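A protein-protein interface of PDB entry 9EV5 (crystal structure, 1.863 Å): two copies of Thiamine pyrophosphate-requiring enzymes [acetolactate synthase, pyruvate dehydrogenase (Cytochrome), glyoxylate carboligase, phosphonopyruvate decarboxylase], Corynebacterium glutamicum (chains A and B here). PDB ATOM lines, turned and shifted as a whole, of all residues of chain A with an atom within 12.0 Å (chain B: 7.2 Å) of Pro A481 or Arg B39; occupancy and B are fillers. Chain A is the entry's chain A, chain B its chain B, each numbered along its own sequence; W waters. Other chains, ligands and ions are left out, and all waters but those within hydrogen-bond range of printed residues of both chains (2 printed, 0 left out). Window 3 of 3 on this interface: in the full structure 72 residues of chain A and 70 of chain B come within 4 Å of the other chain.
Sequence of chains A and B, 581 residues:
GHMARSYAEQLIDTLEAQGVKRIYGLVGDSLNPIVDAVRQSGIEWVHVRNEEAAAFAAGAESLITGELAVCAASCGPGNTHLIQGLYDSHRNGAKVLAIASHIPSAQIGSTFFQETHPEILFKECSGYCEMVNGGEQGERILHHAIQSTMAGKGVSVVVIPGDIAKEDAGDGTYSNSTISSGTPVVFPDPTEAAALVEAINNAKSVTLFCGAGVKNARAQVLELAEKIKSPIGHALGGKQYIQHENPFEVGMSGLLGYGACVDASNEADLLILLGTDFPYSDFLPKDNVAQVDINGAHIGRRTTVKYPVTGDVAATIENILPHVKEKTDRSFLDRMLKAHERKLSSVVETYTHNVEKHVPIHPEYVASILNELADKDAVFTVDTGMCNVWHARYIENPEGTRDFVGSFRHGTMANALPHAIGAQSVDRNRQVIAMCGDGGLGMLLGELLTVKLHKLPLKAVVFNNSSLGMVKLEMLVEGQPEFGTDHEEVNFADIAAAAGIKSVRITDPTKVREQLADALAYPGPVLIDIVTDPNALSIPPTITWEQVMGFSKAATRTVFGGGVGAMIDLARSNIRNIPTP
No position is printed for both chains.
Of the 7 pairs that touch across the chains among the printed residues, none has its exchanged pair printed and touching as well.
Among the printed residues, pairs that only touch across the chains: Gln A480 with Asp B36, Pro A481 with Asp B36, Pro A481 with Arg B39, Phe A483 with Arg B39, Phe A483 with Trp B45, Gln A480 with Val B35 and Phe A483 with Val B35.
Water W1 lies within hydrogen-bond range of the side-chain carboxylate (OD1) of Asp B36 (2.5 Å), the backbone carbonyl oxygen (O) of Pro A481 (2.7 Å), the guanidinium group (NE) of Arg B39 (3.1 Å) and the side-chain amide nitrogen (NE2) of Gln A480 (3.3 Å).
Water W2 lies within hydrogen-bond range of O of Gly A484 (2.7 Å) and NE1 of Trp B45 (2.9 Å).
The backbone NH (N) of Gln A480 sits at hydrogen-bond distance from the backbone carbonyl oxygen (O) of Met A475 (3.1 Å).
The guanidinium group (NH2) of Arg B39 lies within salt-bridge range of the side-chain carboxylate (OD1) of Asp B36, 3.1 Å away.
The side-chain amide oxygen (OE1) of Gln B40 sits close to the side-chain carboxylate (OD2) of Asp B36 (3.4 Å).
Printed residues of chain B within 4 Å of Gln A480: Val B35 and Asp B36.
Of chain B, only Asp B36 and Arg B39 come within 4 Å of Pro A481.
Printed residues of chain B within 4 Å of Phe A483: Val B35, Arg B39 and Trp B45.
Printed residues of chain A within 4 Å of Val B35: Gln A480 (3.9 Å) and Phe A483 (3.9 Å).
Asp B36 touches two residues of chain A.
Ala B37 touches none of the printed residues of chain A.
No residue of chain A comes within 4 Å of Val B38.
Arg B39 touches just these residues of chain A: Pro A481 (3.6 Å) and Phe A483 (3.7 Å).
Gly B42 touches none of the printed residues of chain A.
Of the printed residues of chain A, Trp B45 touches Phe A483 (3.8 Å).
Of the 13 printed residues of chain B, 4 touch a printed residue of chain A.
Printed residues of chain B that touch a printed residue of chain A: Val B35, Asp B36, Arg B39 and Trp B45.
Hydrophobic or aromatic side chains of chain B that line the printed part of chain A: Val B35 and Trp B45.
Along chain B the printed residues that touch a printed residue of chain A span positions 35 to 45.
Among the printed residues, 7 pairs touch across the chains.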
ATOM      1  N   SER A 467      -6.593   4.808 -18.565  1.00  0.00           N
ATOM      2  CA  SER A 467      -5.180   4.757 -18.266  1.00  0.00           C
ATOM      3  C   SER A 467      -4.926   4.191 -16.889  1.00  0.00           C
ATOM      4  O   SER A 467      -5.790   4.228 -16.000  1.00  0.00           O
ATOM      5  CB  SER A 467      -4.606   6.178 -18.342  1.00  0.00           C
ATOM      6  OG  SER A 467      -3.239   6.299 -17.974  1.00  0.00           O
ATOM      7  N   LEU A 468      -3.687   3.690 -16.715  1.00  0.00           N
ATOM      8  CA  LEU A 468      -3.132   3.289 -15.439  1.00  0.00           C
ATOM      9  C   LEU A 468      -2.467   4.609 -15.069  1.00  0.00           C
ATOM     10  O   LEU A 468      -1.276   4.802 -15.334  1.00  0.00           O
ATOM     11  CB  LEU A 468      -2.084   2.189 -15.647  1.00  0.00           C
ATOM     12  CG  LEU A 468      -2.629   0.875 -16.215  1.00  0.00           C
ATOM     13  CD1 LEU A 468      -1.482  -0.123 -16.464  1.00  0.00           C
ATOM     14  CD2 LEU A 468      -3.675   0.249 -15.272  1.00  0.00           C
ATOM     15  N   MET A 470      -1.539   6.370 -12.414  1.00  0.00           N
ATOM     16  CA  MET A 470      -0.382   6.461 -11.528  1.00  0.00           C
ATOM     17  C   MET A 470       0.897   6.001 -12.254  1.00  0.00           C
ATOM     18  O   MET A 470       1.965   6.574 -12.016  1.00  0.00           O
ATOM     19  CB  MET A 470      -0.634   5.667 -10.215  1.00  0.00           C
ATOM     20  CG  MET A 470       0.477   5.789  -9.145  1.00  0.00           C
ATOM     21  SD  MET A 470       0.755   7.502  -8.611  1.00  0.00           S
ATOM     22  CE  MET A 470      -0.460   7.632  -7.268  1.00  0.00           C
ATOM     23  N   VAL A 471       0.793   4.999 -13.146  1.00  0.00           N
ATOM     24  CA  VAL A 471       1.961   4.519 -13.899  1.00  0.00           C
ATOM     25  C   VAL A 471       2.416   5.548 -14.942  1.00  0.00           C
ATOM     26  O   VAL A 471       3.611   5.724 -15.171  1.00  0.00           O
ATOM     27  CB  VAL A 471       1.733   3.151 -14.560  1.00  0.00           C
ATOM     28  CG1 VAL A 471       3.017   2.675 -15.242  1.00  0.00           C
ATOM     29  CG2 VAL A 471       1.248   2.133 -13.529  1.00  0.00           C
ATOM     30  N   LYS A 472       1.464   6.243 -15.552  1.00  0.00           N
ATOM     31  CA  LYS A 472       1.752   7.303 -16.516  1.00  0.00           C
ATOM     32  C   LYS A 472       2.585   8.410 -15.825  1.00  0.00           C
ATOM     33  O   LYS A 472       3.561   8.891 -16.402  1.00  0.00           O
ATOM     34  CB  LYS A 472       0.438   7.863 -17.071  1.00  0.00           C
ATOM     35  CG  LYS A 472       0.628   8.906 -18.132  1.00  0.00           C
ATOM     36  CD  LYS A 472      -0.700   9.294 -18.736  1.00  0.00           C
ATOM     37  CE  LYS A 472      -0.583   9.333 -20.239  1.00  0.00           C
ATOM     38  NZ  LYS A 472      -1.814   9.844 -20.884  1.00  0.00           N
ATOM     39  N   LEU A 473       2.241   8.726 -14.558  1.00  0.00           N
ATOM     40  CA  LEU A 473       2.970   9.683 -13.711  1.00  0.00           C
ATOM     41  C   LEU A 473       4.412   9.160 -13.491  1.00  0.00           C
ATOM     42  O   LEU A 473       5.359   9.921 -13.654  1.00  0.00           O
ATOM     43  CB  LEU A 473       2.241   9.831 -12.352  1.00  0.00           C
ATOM     44  CG  LEU A 473       2.800  10.835 -11.325  1.00  0.00           C
ATOM     45  CD1 LEU A 473       1.696  11.304 -10.370  1.00  0.00           C
ATOM     46  CD2 LEU A 473       3.932  10.243 -10.516  1.00  0.00           C
ATOM     47  N   GLU A 474       4.570   7.865 -13.123  1.00  0.00           N
ATOM     48  CA  GLU A 474       5.879   7.253 -12.880  1.00  0.00           C
ATOM     49  C   GLU A 474       6.777   7.346 -14.107  1.00  0.00           C
ATOM     50  O   GLU A 474       7.950   7.714 -13.964  1.00  0.00           O
ATOM     51  CB  GLU A 474       5.742   5.778 -12.462  1.00  0.00           C
ATOM     52  CG  GLU A 474       4.950   5.561 -11.183  1.00  0.00           C
ATOM     53  CD  GLU A 474       4.560   4.115 -10.918  1.00  0.00           C
ATOM     54  OE1 GLU A 474       4.644   3.282 -11.851  1.00  0.00           O
ATOM     55  OE2 GLU A 474       4.177   3.817  -9.765  1.00  0.00           O
ATOM     56  N   MET A 475       6.224   7.056 -15.316  1.00  0.00           N
ATOM     57  CA  MET A 475       7.013   7.128 -16.544  1.00  0.00           C
ATOM     58  C   MET A 475       7.389   8.560 -16.917  1.00  0.00           C
ATOM     59  O   MET A 475       8.457   8.800 -17.496  1.00  0.00           O
ATOM     60  CB  MET A 475       6.294   6.444 -17.700  1.00  0.00           C
ATOM     61  CG  MET A 475       6.068   4.980 -17.438  1.00  0.00           C
ATOM     62  SD  MET A 475       5.363   4.150 -18.860  1.00  0.00           S
ATOM     63  CE  MET A 475       5.297   2.460 -18.211  1.00  0.00           C
ATOM     64  N   LEU A 476       6.516   9.510 -16.595  1.00  0.00           N
ATOM     65  CA  LEU A 476       6.746  10.932 -16.846  1.00  0.00           C
ATOM     66  C   LEU A 476       7.949  11.378 -16.013  1.00  0.00           C
ATOM     67  O   LEU A 476       8.868  11.990 -16.552  1.00  0.00           O
ATOM     68  CB  LEU A 476       5.488  11.718 -16.434  1.00  0.00           C
ATOM     69  CG  LEU A 476       5.230  12.975 -17.164  1.00  0.00           C
ATOM     70  CD1 LEU A 476       4.730  12.677 -18.571  1.00  0.00           C
ATOM     71  CD2 LEU A 476       4.239  13.848 -16.396  1.00  0.00           C
ATOM     72  N   VAL A 477       7.982  10.969 -14.729  1.00  0.00           N
ATOM     73  CA  VAL A 477       9.038  11.292 -13.768  1.00  0.00           C
ATOM     74  C   VAL A 477      10.375  10.647 -14.172  1.00  0.00           C
ATOM     75  O   VAL A 477      11.445  11.255 -14.015  1.00  0.00           O
ATOM     76  CB  VAL A 477       8.552  10.843 -12.370  1.00  0.00           C
ATOM     77  CG1 VAL A 477       9.689  10.647 -11.396  1.00  0.00           C
ATOM     78  CG2 VAL A 477       7.528  11.813 -11.810  1.00  0.00           C
ATOM     79  N   GLU A 478      10.319   9.420 -14.680  1.00  0.00           N
ATOM     80  CA  GLU A 478      11.521   8.704 -15.121  1.00  0.00           C
ATOM     81  C   GLU A 478      12.071   9.273 -16.428  1.00  0.00           C
ATOM     82  O   GLU A 478      13.273   9.248 -16.634  1.00  0.00           O
ATOM     83  CB  GLU A 478      11.197   7.202 -15.290  1.00  0.00           C
ATOM     84  CG  GLU A 478      12.292   6.357 -15.916  1.00  0.00           C
ATOM     85  CD  GLU A 478      13.462   6.019 -15.006  1.00  0.00           C
ATOM     86  OE1 GLU A 478      13.399   4.964 -14.332  1.00  0.00           O
ATOM     87  OE2 GLU A 478      14.444   6.798 -14.982  1.00  0.00           O
ATOM     88  N   GLY A 479      11.203   9.822 -17.275  1.00  0.00           N
ATOM     89  CA  GLY A 479      11.583  10.310 -18.588  1.00  0.00           C
ATOM     90  C   GLY A 479      11.422   9.257 -19.678  1.00  0.00           C
ATOM     91  O   GLY A 479      11.799   9.486 -20.829  1.00  0.00           O
ATOM     92  N   GLN A 480      10.815   8.115 -19.337  1.00  0.00           N
ATOM     93  CA  GLN A 480      10.535   6.985 -20.187  1.00  0.00           C
ATOM     94  C   GLN A 480       9.343   7.305 -21.080  1.00  0.00           C
ATOM     95  O   GLN A 480       8.327   7.794 -20.596  1.00  0.00           O
ATOM     96  CB  GLN A 480      10.202   5.822 -19.241  1.00  0.00           C
ATOM     97  CG  GLN A 480       9.389   4.652 -19.782  1.00  0.00           C
ATOM     98  CD  GLN A 480       9.383   3.474 -18.816  1.00  0.00           C
ATOM     99  OE1 GLN A 480      10.065   3.467 -17.783  1.00  0.00           O
ATOM    100  NE2 GLN A 480       8.628   2.436 -19.141  1.00  0.00           N
ATOM    101  N   PRO A 481       9.436   7.007 -22.386  1.00  0.00           N
ATOM    102  CA  PRO A 481       8.295   7.253 -23.279  1.00  0.00           C
ATOM    103  C   PRO A 481       7.059   6.454 -22.861  1.00  0.00           C
ATOM    104  O   PRO A 481       7.157   5.274 -22.527  1.00  0.00           O
ATOM    105  CB  PRO A 481       8.810   6.791 -24.651  1.00  0.00           C
ATOM    106  CG  PRO A 481      10.287   6.733 -24.527  1.00  0.00           C
ATOM    107  CD  PRO A 481      10.575   6.406 -23.103  1.00  0.00           C
ATOM    108  N   GLU A 482       5.896   7.109 -22.876  1.00  0.00           N
ATOM    109  CA  GLU A 482       4.626   6.517 -22.475  1.00  0.00           C
ATOM    110  C   GLU A 482       4.310   5.246 -23.260  1.00  0.00           C
ATOM    111  O   GLU A 482       4.248   5.285 -24.480  1.00  0.00           O
ATOM    112  CB  GLU A 482       3.503   7.552 -22.619  1.00  0.00           C
ATOM    113  CG  GLU A 482       2.195   7.115 -21.996  1.00  0.00           C
ATOM    114  CD  GLU A 482       1.015   7.452 -22.876  1.00  0.00           C
ATOM    115  OE1 GLU A 482       0.190   6.544 -23.127  1.00  0.00           O
ATOM    116  OE2 GLU A 482       0.932   8.612 -23.345  1.00  0.00           O
ATOM    117  N   PHE A 483       4.175   4.107 -22.563  1.00  0.00           N
ATOM    118  CA  PHE A 483       3.902   2.841 -23.223  1.00  0.00           C
ATOM    119  C   PHE A 483       3.278   1.862 -22.221  1.00  0.00           C
ATOM    120  O   PHE A 483       3.785   1.725 -21.102  1.00  0.00           O
ATOM    121  CB  PHE A 483       5.208   2.248 -23.790  1.00  0.00           C
ATOM    122  CG  PHE A 483       5.063   0.895 -24.454  1.00  0.00           C
ATOM    123  CD1 PHE A 483       4.613   0.790 -25.757  1.00  0.00           C
ATOM    124  CD2 PHE A 483       5.401  -0.266 -23.781  1.00  0.00           C
ATOM    125  CE1 PHE A 483       4.514  -0.450 -26.373  1.00  0.00           C
ATOM    126  CE2 PHE A 483       5.267  -1.507 -24.388  1.00  0.00           C
ATOM    127  CZ  PHE A 483       4.839  -1.593 -25.682  1.00  0.00           C
ATOM    128  N   GLY A 484       2.210   1.180 -22.643  1.00  0.00           N
ATOM    129  CA  GLY A 484       1.556   0.162 -21.827  1.00  0.00           C
ATOM    130  C   GLY A 484       0.599   0.668 -20.773  1.00  0.00           C
ATOM    131  O   GLY A 484       0.001  -0.130 -20.048  1.00  0.00           O
ATOM    132  N   THR A 485       0.392   1.992 -20.714  1.00  0.00           N
ATOM    133  CA  THR A 485      -0.475   2.575 -19.702  1.00  0.00           C
ATOM    134  C   THR A 485      -1.863   2.980 -20.211  1.00  0.00           C
ATOM    135  O   THR A 485      -2.836   2.849 -19.471  1.00  0.00           O
ATOM    136  CB  THR A 485       0.235   3.768 -19.040  1.00  0.00           C
ATOM    137  OG1 THR A 485       0.360   4.824 -19.988  1.00  0.00           O
ATOM    138  CG2 THR A 485       1.592   3.399 -18.481  1.00  0.00           C
ATOM    139  N   ASP A 486      -1.934   3.536 -21.440  1.00  0.00           N
ATOM    140  CA  ASP A 486      -3.166   4.059 -22.034  1.00  0.00           C
ATOM    141  C   ASP A 486      -3.697   3.184 -23.158  1.00  0.00           C
ATOM    142  O   ASP A 486      -2.953   2.775 -24.055  1.00  0.00           O
ATOM    143  CB  ASP A 486      -2.956   5.500 -22.546  1.00  0.00           C
ATOM    144  CG  ASP A 486      -2.739   6.497 -21.432  1.00  0.00           C
ATOM    145  OD1 ASP A 486      -2.009   6.157 -20.460  1.00  0.00           O
ATOM    146  OD2 ASP A 486      -3.295   7.630 -21.530  1.00  0.00           O
ATOM    147  N   HIS A 487      -4.988   2.883 -23.103  1.00  0.00           N
ATOM    148  CA  HIS A 487      -5.604   1.992 -24.073  1.00  0.00           C
ATOM    149  C   HIS A 487      -6.965   2.544 -24.505  1.00  0.00           C
ATOM    150  O   HIS A 487      -7.428   3.561 -23.956  1.00  0.00           O
ATOM    151  CB  HIS A 487      -5.712   0.549 -23.485  1.00  0.00           C
ATOM    152  CG  HIS A 487      -4.414   0.023 -22.958  1.00  0.00           C
ATOM    153  ND1 HIS A 487      -4.088   0.121 -21.615  1.00  0.00           N
ATOM    154  CD2 HIS A 487      -3.388  -0.574 -23.609  1.00  0.00           C
ATOM    155  CE1 HIS A 487      -2.896  -0.429 -21.495  1.00  0.00           C
ATOM    156  NE2 HIS A 487      -2.438  -0.855 -22.671  1.00  0.00           N
ATOM    157  N   ASN A 535      -4.027  13.062 -18.301  1.00  0.00           N
ATOM    158  CA  ASN A 535      -2.897  13.981 -18.239  1.00  0.00           C
ATOM    159  C   ASN A 535      -3.098  15.093 -17.211  1.00  0.00           C
ATOM    160  O   ASN A 535      -2.401  16.112 -17.291  1.00  0.00           O
ATOM    161  CB  ASN A 535      -2.606  14.592 -19.605  1.00  0.00           C
ATOM    162  CG  ASN A 535      -2.465  13.544 -20.676  1.00  0.00           C
ATOM    163  OD1 ASN A 535      -1.606  12.659 -20.623  1.00  0.00           O
ATOM    164  ND2 ASN A 535      -3.339  13.595 -21.663  1.00  0.00           N
ATOM    165  N   LEU A 537      -1.933  16.033 -14.479  1.00  0.00           N
ATOM    166  CA  LEU A 537      -0.744  15.771 -13.687  1.00  0.00           C
ATOM    167  C   LEU A 537       0.146  17.009 -13.748  1.00  0.00           C
ATOM    168  O   LEU A 537       0.372  17.571 -14.827  1.00  0.00           O
ATOM    169  CB  LEU A 537       0.059  14.610 -14.316  1.00  0.00           C
ATOM    170  CG  LEU A 537      -0.556  13.232 -14.290  1.00  0.00           C
ATOM    171  CD1 LEU A 537       0.237  12.259 -15.193  1.00  0.00           C
ATOM    172  CD2 LEU A 537      -0.659  12.715 -12.860  1.00  0.00           C
ATOM    173  N   TRP A 545      12.748   9.055 -10.334  1.00  0.00           N
ATOM    174  CA  TRP A 545      12.147   7.719 -10.268  1.00  0.00           C
ATOM    175  C   TRP A 545      12.394   7.080  -8.910  1.00  0.00           C
ATOM    176  O   TRP A 545      11.486   6.472  -8.364  1.00  0.00           O
ATOM    177  CB  TRP A 545      12.652   6.790 -11.393  1.00  0.00           C
ATOM    178  CG  TRP A 545      11.767   5.585 -11.588  1.00  0.00           C
ATOM    179  CD1 TRP A 545      10.488   5.575 -12.060  1.00  0.00           C
ATOM    180  CD2 TRP A 545      12.089   4.222 -11.268  1.00  0.00           C
ATOM    181  NE1 TRP A 545       9.995   4.280 -12.077  1.00  0.00           N
ATOM    182  CE2 TRP A 545      10.973   3.429 -11.626  1.00  0.00           C
ATOM    183  CE3 TRP A 545      13.226   3.591 -10.758  1.00  0.00           C
ATOM    184  CZ2 TRP A 545      10.950   2.043 -11.442  1.00  0.00           C
ATOM    185  CZ3 TRP A 545      13.207   2.218 -10.587  1.00  0.00           C
ATOM    186  CH2 TRP A 545      12.076   1.461 -10.921  1.00  0.00           C
ATOM    187  N   ILE B  12      15.446  -8.683 -21.477  1.00  0.00           N
ATOM    188  CA  ILE B  12      14.615  -8.677 -22.679  1.00  0.00           C
ATOM    189  C   ILE B  12      15.392  -9.161 -23.912  1.00  0.00           C
ATOM    190  O   ILE B  12      14.833  -9.909 -24.709  1.00  0.00           O
ATOM    191  CB  ILE B  12      13.927  -7.310 -22.884  1.00  0.00           C
ATOM    192  CG1 ILE B  12      12.894  -7.058 -21.778  1.00  0.00           C
ATOM    193  CG2 ILE B  12      13.262  -7.228 -24.233  1.00  0.00           C
ATOM    194  CD1 ILE B  12      11.853  -8.200 -21.553  1.00  0.00           C
ATOM    195  N   ILE B  34      11.574  -2.749 -17.373  1.00  0.00           N
ATOM    196  CA  ILE B  34      11.465  -3.941 -18.186  1.00  0.00           C
ATOM    197  C   ILE B  34      10.523  -3.718 -19.368  1.00  0.00           C
ATOM    198  O   ILE B  34      10.868  -4.087 -20.497  1.00  0.00           O
ATOM    199  CB  ILE B  34      11.062  -5.160 -17.340  1.00  0.00           C
ATOM    200  CG1 ILE B  34      12.158  -5.457 -16.288  1.00  0.00           C
ATOM    201  CG2 ILE B  34      10.813  -6.382 -18.227  1.00  0.00           C
ATOM    202  CD1 ILE B  34      11.775  -6.446 -15.248  1.00  0.00           C
ATOM    203  N   VAL B  35       9.353  -3.086 -19.136  1.00  0.00           N
ATOM    204  CA  VAL B  35       8.437  -2.827 -20.243  1.00  0.00           C
ATOM    205  C   VAL B  35       9.029  -1.793 -21.228  1.00  0.00           C
ATOM    206  O   VAL B  35       8.734  -1.880 -22.424  1.00  0.00           O
ATOM    207  CB  VAL B  35       6.994  -2.491 -19.826  1.00  0.00           C
ATOM    208  CG1 VAL B  35       6.509  -3.408 -18.706  1.00  0.00           C
ATOM    209  CG2 VAL B  35       6.842  -1.027 -19.486  1.00  0.00           C
ATOM    210  N   ASP B  36       9.903  -0.887 -20.761  1.00  0.00           N
ATOM    211  CA  ASP B  36      10.556   0.059 -21.665  1.00  0.00           C
ATOM    212  C   ASP B  36      11.478  -0.693 -22.637  1.00  0.00           C
ATOM    213  O   ASP B  36      11.528  -0.360 -23.829  1.00  0.00           O
ATOM    214  CB  ASP B  36      11.366   1.107 -20.909  1.00  0.00           C
ATOM    215  CG  ASP B  36      11.833   2.188 -21.854  1.00  0.00           C
ATOM    216  OD1 ASP B  36      10.977   2.962 -22.328  1.00  0.00           O
ATOM    217  OD2 ASP B  36      13.050   2.227 -22.162  1.00  0.00           O
ATOM    218  N   ALA B  37      12.181  -1.720 -22.127  1.00  0.00           N
ATOM    219  CA  ALA B  37      13.031  -2.561 -22.945  1.00  0.00           C
ATOM    220  C   ALA B  37      12.158  -3.401 -23.925  1.00  0.00           C
ATOM    221  O   ALA B  37      12.519  -3.535 -25.093  1.00  0.00           O
ATOM    222  CB  ALA B  37      13.887  -3.455 -22.054  1.00  0.00           C
ATOM    223  N   VAL B  38      10.974  -3.876 -23.483  1.00  0.00           N
ATOM    224  CA  VAL B  38      10.021  -4.617 -24.331  1.00  0.00           C
ATOM    225  C   VAL B  38       9.628  -3.750 -25.514  1.00  0.00           C
ATOM    226  O   VAL B  38       9.721  -4.209 -26.645  1.00  0.00           O
ATOM    227  CB  VAL B  38       8.756  -5.107 -23.555  1.00  0.00           C
ATOM    228  CG1 VAL B  38       7.693  -5.643 -24.500  1.00  0.00           C
ATOM    229  CG2 VAL B  38       9.111  -6.160 -22.516  1.00  0.00           C
ATOM    230  N   ARG B  39       9.260  -2.480 -25.252  1.00  0.00           N
ATOM    231  CA  ARG B  39       8.888  -1.489 -26.261  1.00  0.00           C
ATOM    232  C   ARG B  39       9.981  -1.357 -27.338  1.00  0.00           C
ATOM    233  O   ARG B  39       9.674  -1.406 -28.527  1.00  0.00           O
ATOM    234  CB  ARG B  39       8.637  -0.127 -25.589  1.00  0.00           C
ATOM    235  CG  ARG B  39       8.343   1.000 -26.571  1.00  0.00           C
ATOM    236  CD  ARG B  39       8.329   2.362 -25.901  1.00  0.00           C
ATOM    237  NE  ARG B  39       9.621   2.696 -25.301  1.00  0.00           N
ATOM    238  CZ  ARG B  39      10.608   3.318 -25.941  1.00  0.00           C
ATOM    239  NH1 ARG B  39      10.464   3.673 -27.214  1.00  0.00           N
ATOM    240  NH2 ARG B  39      11.748   3.585 -25.317  1.00  0.00           N
ATOM    241  N   GLN B  40      11.252  -1.266 -26.928  1.00  0.00           N
ATOM    242  CA  GLN B  40      12.362  -1.154 -27.871  1.00  0.00           C
ATOM    243  C   GLN B  40      12.704  -2.456 -28.611  1.00  0.00           C
ATOM    244  O   GLN B  40      13.382  -2.425 -29.629  1.00  0.00           O
ATOM    245  CB  GLN B  40      13.591  -0.606 -27.155  1.00  0.00           C
ATOM    246  CG  GLN B  40      13.350   0.790 -26.602  1.00  0.00           C
ATOM    247  CD  GLN B  40      14.617   1.453 -26.131  1.00  0.00           C
ATOM    248  OE1 GLN B  40      14.859   1.615 -24.940  1.00  0.00           O
ATOM    249  NE2 GLN B  40      15.462   1.851 -27.061  1.00  0.00           N
ATOM    250  N   SER B  41      12.231  -3.589 -28.124  1.00  0.00           N
ATOM    251  CA  SER B  41      12.514  -4.888 -28.710  1.00  0.00           C
ATOM    252  C   SER B  41      11.436  -5.336 -29.711  1.00  0.00           C
ATOM    253  O   SER B  41      10.407  -4.679 -29.866  1.00  0.00           O
ATOM    254  CB  SER B  41      12.662  -5.919 -27.591  1.00  0.00           C
ATOM    255  OG  SER B  41      11.391  -6.332 -27.119  1.00  0.00           O
ATOM    256  N   GLY B  42      11.675  -6.456 -30.376  1.00  0.00           N
ATOM    257  CA  GLY B  42      10.685  -7.060 -31.262  1.00  0.00           C
ATOM    258  C   GLY B  42       9.642  -7.895 -30.513  1.00  0.00           C
ATOM    259  O   GLY B  42       8.769  -8.488 -31.139  1.00  0.00           O
ATOM    260  N   ILE B  43       9.705  -7.957 -29.159  1.00  0.00           N
ATOM    261  CA  ILE B  43       8.699  -8.675 -28.376  1.00  0.00           C
ATOM    262  C   ILE B  43       7.424  -7.789 -28.225  1.00  0.00           C
ATOM    263  O   ILE B  43       7.524  -6.567 -28.108  1.00  0.00           O
ATOM    264  CB  ILE B  43       9.292  -9.096 -27.011  1.00  0.00           C
ATOM    265  CG1 ILE B  43      10.423 -10.114 -27.186  1.00  0.00           C
ATOM    266  CG2 ILE B  43       8.231  -9.611 -26.044  1.00  0.00           C
ATOM    267  CD1 ILE B  43      11.170 -10.449 -25.888  1.00  0.00           C
ATOM    268  N   GLU B  44       6.247  -8.393 -28.263  1.00  0.00           N
ATOM    269  CA  GLU B  44       5.004  -7.647 -28.103  1.00  0.00           C
ATOM    270  C   GLU B  44       4.580  -7.626 -26.620  1.00  0.00           C
ATOM    271  O   GLU B  44       4.747  -8.614 -25.926  1.00  0.00           O
ATOM    272  CB  GLU B  44       3.901  -8.199 -29.023  1.00  0.00           C
ATOM    273  CG  GLU B  44       2.585  -7.474 -28.832  1.00  0.00           C
ATOM    274  CD  GLU B  44       1.398  -7.897 -29.677  1.00  0.00           C
ATOM    275  OE1 GLU B  44       0.332  -7.253 -29.543  1.00  0.00           O
ATOM    276  OE2 GLU B  44       1.525  -8.863 -30.466  1.00  0.00           O
ATOM    277  N   TRP B  45       4.058  -6.492 -26.132  1.00  0.00           N
ATOM    278  CA  TRP B  45       3.580  -6.386 -24.761  1.00  0.00           C
ATOM    279  C   TRP B  45       2.084  -6.596 -24.808  1.00  0.00           C
ATOM    280  O   TRP B  45       1.397  -5.911 -25.559  1.00  0.00           O
ATOM    281  CB  TRP B  45       3.909  -5.002 -24.172  1.00  0.00           C
ATOM    282  CG  TRP B  45       3.400  -4.833 -22.771  1.00  0.00           C
ATOM    283  CD1 TRP B  45       2.323  -4.092 -22.373  1.00  0.00           C
ATOM    284  CD2 TRP B  45       3.883  -5.507 -21.598  1.00  0.00           C
ATOM    285  NE1 TRP B  45       2.108  -4.257 -21.027  1.00  0.00           N
ATOM    286  CE2 TRP B  45       3.054  -5.119 -20.524  1.00  0.00           C
ATOM    287  CE3 TRP B  45       4.931  -6.405 -21.354  1.00  0.00           C
ATOM    288  CZ2 TRP B  45       3.274  -5.554 -19.219  1.00  0.00           C
ATOM    289  CZ3 TRP B  45       5.120  -6.872 -20.063  1.00  0.00           C
ATOM    290  CH2 TRP B  45       4.309  -6.430 -19.009  1.00  0.00           C
HETATM  291  O   HOH W   1       8.444   2.863 -22.432  1.00  0.00           O
HETATM  292  O   HOH W   2       0.254  -2.766 -19.315  1.00  0.00           O
